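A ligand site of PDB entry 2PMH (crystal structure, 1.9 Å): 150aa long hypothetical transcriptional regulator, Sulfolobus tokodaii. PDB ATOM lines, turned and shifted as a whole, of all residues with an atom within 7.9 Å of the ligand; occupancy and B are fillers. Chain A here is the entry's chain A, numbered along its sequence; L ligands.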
ATOM      1  N   LEU A  20      11.844 -15.540 -12.288  1.00  0.00           N
ATOM      2  CA  LEU A  20      11.594 -16.244 -13.542  1.00  0.00           C
ATOM      3  C   LEU A  20      12.556 -15.822 -14.643  1.00  0.00           C
ATOM      4  O   LEU A  20      12.944 -16.627 -15.488  1.00  0.00           O
ATOM      5  CB  LEU A  20      10.154 -16.010 -13.997  1.00  0.00           C
ATOM      6  CG  LEU A  20       9.065 -16.729 -13.189  1.00  0.00           C
ATOM      7  CD1 LEU A  20       7.694 -16.405 -13.762  1.00  0.00           C
ATOM      8  CD2 LEU A  20       9.314 -18.234 -13.230  1.00  0.00           C
ATOM      9  N   ASP A  21      12.949 -14.548 -14.634  1.00  0.00           N
ATOM     10  CA  ASP A  21      13.876 -14.033 -15.632  1.00  0.00           C
ATOM     11  C   ASP A  21      15.253 -14.655 -15.495  1.00  0.00           C
ATOM     12  O   ASP A  21      15.873 -15.035 -16.483  1.00  0.00           O
ATOM     13  CB  ASP A  21      13.981 -12.509 -15.534  1.00  0.00           C
ATOM     14  CG  ASP A  21      12.794 -11.804 -16.140  1.00  0.00           C
ATOM     15  OD1 ASP A  21      12.549 -12.010 -17.348  1.00  0.00           O
ATOM     16  OD2 ASP A  21      12.112 -11.056 -15.417  1.00  0.00           O
ATOM     17  N   GLU A  22      15.731 -14.747 -14.254  1.00  0.00           N
ATOM     18  CA  GLU A  22      17.041 -15.331 -14.014  1.00  0.00           C
ATOM     19  C   GLU A  22      17.008 -16.820 -14.367  1.00  0.00           C
ATOM     20  O   GLU A  22      17.976 -17.353 -14.936  1.00  0.00           O
ATOM     21  CB  GLU A  22      17.450 -15.138 -12.545  1.00  0.00           C
ATOM     22  CG  GLU A  22      17.816 -13.698 -12.199  1.00  0.00           C
ATOM     23  CD  GLU A  22      18.224 -13.542 -10.749  1.00  0.00           C
ATOM     24  OE1 GLU A  22      17.383 -13.804  -9.851  1.00  0.00           O
ATOM     25  OE2 GLU A  22      19.393 -13.155 -10.493  1.00  0.00           O
ATOM     26  N   ILE A  23      15.905 -17.484 -14.039  1.00  0.00           N
ATOM     27  CA  ILE A  23      15.764 -18.916 -14.333  1.00  0.00           C
ATOM     28  C   ILE A  23      15.643 -19.111 -15.844  1.00  0.00           C
ATOM     29  O   ILE A  23      16.365 -19.913 -16.430  1.00  0.00           O
ATOM     30  CB  ILE A  23      14.503 -19.502 -13.655  1.00  0.00           C
ATOM     31  CG1 ILE A  23      14.569 -19.302 -12.142  1.00  0.00           C
ATOM     32  CG2 ILE A  23      14.399 -20.989 -13.966  1.00  0.00           C
ATOM     33  CD1 ILE A  23      13.351 -19.809 -11.397  1.00  0.00           C
ATOM     34  N   ALA A  24      14.724 -18.366 -16.464  1.00  0.00           N
ATOM     35  CA  ALA A  24      14.503 -18.456 -17.899  1.00  0.00           C
ATOM     36  C   ALA A  24      15.783 -18.145 -18.670  1.00  0.00           C
ATOM     37  O   ALA A  24      16.004 -18.672 -19.758  1.00  0.00           O
ATOM     38  CB  ALA A  24      13.409 -17.481 -18.315  1.00  0.00           C
ATOM     39  N   ARG A  25      16.634 -17.295 -18.086  1.00  0.00           N
ATOM     40  CA  ARG A  25      17.889 -16.902 -18.705  1.00  0.00           C
ATOM     41  C   ARG A  25      18.971 -17.974 -18.550  1.00  0.00           C
ATOM     42  O   ARG A  25      19.856 -18.108 -19.393  1.00  0.00           O
ATOM     43  CB  ARG A  25      18.380 -15.587 -18.086  1.00  0.00           C
ATOM     44  CG  ARG A  25      19.667 -15.015 -18.700  1.00  0.00           C
ATOM     45  CD  ARG A  25      20.096 -13.760 -17.957  1.00  0.00           C
ATOM     46  NE  ARG A  25      19.012 -12.783 -17.878  1.00  0.00           N
ATOM     47  CZ  ARG A  25      18.628 -12.154 -16.765  1.00  0.00           C
ATOM     48  NH1 ARG A  25      19.257 -12.406 -15.612  1.00  0.00           N
ATOM     49  NH2 ARG A  25      17.630 -11.292 -16.805  1.00  0.00           N
ATOM     50  N   ARG A  28      17.484 -20.911 -20.758  1.00  0.00           N
ATOM     51  CA  ARG A  28      17.297 -20.472 -22.140  1.00  0.00           C
ATOM     52  C   ARG A  28      15.934 -20.753 -22.779  1.00  0.00           C
ATOM     53  O   ARG A  28      15.861 -21.354 -23.850  1.00  0.00           O
ATOM     54  CB  ARG A  28      18.386 -21.072 -23.031  1.00  0.00           C
ATOM     55  CG  ARG A  28      19.766 -20.450 -22.841  1.00  0.00           C
ATOM     56  CD  ARG A  28      19.727 -18.978 -23.216  1.00  0.00           C
ATOM     57  NE  ARG A  28      21.048 -18.357 -23.157  1.00  0.00           N
ATOM     58  CZ  ARG A  28      21.269 -17.075 -23.430  1.00  0.00           C
ATOM     59  NH1 ARG A  28      22.488 -16.572 -23.356  1.00  0.00           N
ATOM     60  NH2 ARG A  28      20.257 -16.278 -23.777  1.00  0.00           N
ATOM     61  N   ILE A  29      14.849 -20.313 -22.137  1.00  0.00           N
ATOM     62  CA  ILE A  29      13.512 -20.521 -22.692  1.00  0.00           C
ATOM     63  C   ILE A  29      12.578 -19.362 -22.346  1.00  0.00           C
ATOM     64  O   ILE A  29      12.814 -18.634 -21.379  1.00  0.00           O
ATOM     65  CB  ILE A  29      12.864 -21.834 -22.183  1.00  0.00           C
ATOM     66  CG1 ILE A  29      12.471 -21.698 -20.714  1.00  0.00           C
ATOM     67  CG2 ILE A  29      13.825 -23.001 -22.376  1.00  0.00           C
ATOM     68  CD1 ILE A  29      11.614 -22.843 -20.212  1.00  0.00           C
ATOM     69  N   PRO A  30      11.503 -19.180 -23.130  1.00  0.00           N
ATOM     70  CA  PRO A  30      10.544 -18.099 -22.891  1.00  0.00           C
ATOM     71  C   PRO A  30      10.011 -18.110 -21.465  1.00  0.00           C
ATOM     72  O   PRO A  30       9.410 -19.087 -21.031  1.00  0.00           O
ATOM     73  CB  PRO A  30       9.449 -18.384 -23.919  1.00  0.00           C
ATOM     74  CG  PRO A  30      10.219 -18.971 -25.050  1.00  0.00           C
ATOM     75  CD  PRO A  30      11.157 -19.926 -24.343  1.00  0.00           C
ATOM     76  N   LYS A  31      10.234 -17.013 -20.751  1.00  0.00           N
ATOM     77  CA  LYS A  31       9.783 -16.902 -19.364  1.00  0.00           C
ATOM     78  C   LYS A  31       8.314 -17.288 -19.229  1.00  0.00           C
ATOM     79  O   LYS A  31       7.873 -17.751 -18.178  1.00  0.00           O
ATOM     80  CB  LYS A  31       9.971 -15.471 -18.857  1.00  0.00           C
ATOM     81  CG  LYS A  31       9.686 -15.307 -17.372  1.00  0.00           C
ATOM     82  CD  LYS A  31       9.384 -13.863 -17.012  1.00  0.00           C
ATOM     83  CE  LYS A  31       8.123 -13.400 -17.710  1.00  0.00           C
ATOM     84  NZ  LYS A  31       7.016 -14.387 -17.533  1.00  0.00           N
ATOM     85  N   SER A  32       7.552 -17.100 -20.309  1.00  0.00           N
ATOM     86  CA  SER A  32       6.140 -17.441 -20.320  1.00  0.00           C
ATOM     87  C   SER A  32       5.937 -18.955 -20.297  1.00  0.00           C
ATOM     88  O   SER A  32       4.996 -19.453 -19.677  1.00  0.00           O
ATOM     89  CB  SER A  32       5.484 -16.853 -21.573  1.00  0.00           C
ATOM     90  OG  SER A  32       6.213 -17.195 -22.741  1.00  0.00           O
ATOM     91  N   THR A  33       6.828 -19.676 -20.967  1.00  0.00           N
ATOM     92  CA  THR A  33       6.768 -21.134 -21.024  1.00  0.00           C
ATOM     93  C   THR A  33       7.226 -21.712 -19.687  1.00  0.00           C
ATOM     94  O   THR A  33       6.564 -22.583 -19.126  1.00  0.00           O
ATOM     95  CB  THR A  33       7.674 -21.679 -22.147  1.00  0.00           C
ATOM     96  OG1 THR A  33       7.207 -21.193 -23.413  1.00  0.00           O
ATOM     97  CG2 THR A  33       7.646 -23.208 -22.156  1.00  0.00           C
ATOM     98  N   LEU A  34       8.360 -21.214 -19.202  1.00  0.00           N
ATOM     99  CA  LEU A  34       8.899 -21.654 -17.922  1.00  0.00           C
ATOM    100  C   LEU A  34       7.768 -21.663 -16.911  1.00  0.00           C
ATOM    101  O   LEU A  34       7.538 -22.654 -16.214  1.00  0.00           O
ATOM    102  CB  LEU A  34       9.998 -20.695 -17.461  1.00  0.00           C
ATOM    103  CG  LEU A  34      10.452 -20.807 -16.003  1.00  0.00           C
ATOM    104  CD1 LEU A  34      10.964 -22.218 -15.722  1.00  0.00           C
ATOM    105  CD2 LEU A  34      11.533 -19.778 -15.728  1.00  0.00           C
HETATM  106  N1  LIG L   1       8.337 -13.957 -24.450  1.00  0.00           N
HETATM  107  C1  LIG L   1       8.561 -14.182 -23.001  1.00  0.00           C
HETATM  108  C2  LIG L   1       7.380 -13.780 -22.140  1.00  0.00           C
HETATM  109  O1  LIG L   1       6.220 -13.959 -22.584  1.00  0.00           O
HETATM  110  C3  LIG L   1       9.815 -13.449 -22.534  1.00  0.00           C
HETATM  111  C4  LIG L   1      11.096 -14.243 -22.718  1.00  0.00           C
HETATM  112  C5  LIG L   1      11.917 -14.320 -21.450  1.00  0.00           C
HETATM  113  O2  LIG L   1      12.859 -15.110 -21.348  1.00  0.00           O
HETATM  114  N2  LIG L   1      11.565 -13.496 -20.471  1.00  0.00           N
HETATM  115  O3  LIG L   1       7.603 -13.284 -21.011  1.00  0.00           O
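O1 of the ligand lies close to OG of Ser 32 (3.2 Å).
O2 of the ligand sits close to N of Lys 31 (3.3 Å).
NZ of Lys 31 lies within salt-bridge range of O3 of the ligand (3.7 Å).
The backbone carbonyl oxygen of Ala 24 sits at hydrogen-bond distance from the backbone NH of Ile 29 (3.1 Å).
Asp 21 touches the ligand.
CB of Ala 24 touches O2 of the ligand, at 3.9 Å.
O of Ile 29 touches O2 of the ligand, 3.5 Å away.
Pro 30 touches the ligand.
Hydrophobic or aromatic side chains that line the ligand: Ala 24.
The nearest printed residue that does not touch the ligand is Arg 25 (5.4 Å).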
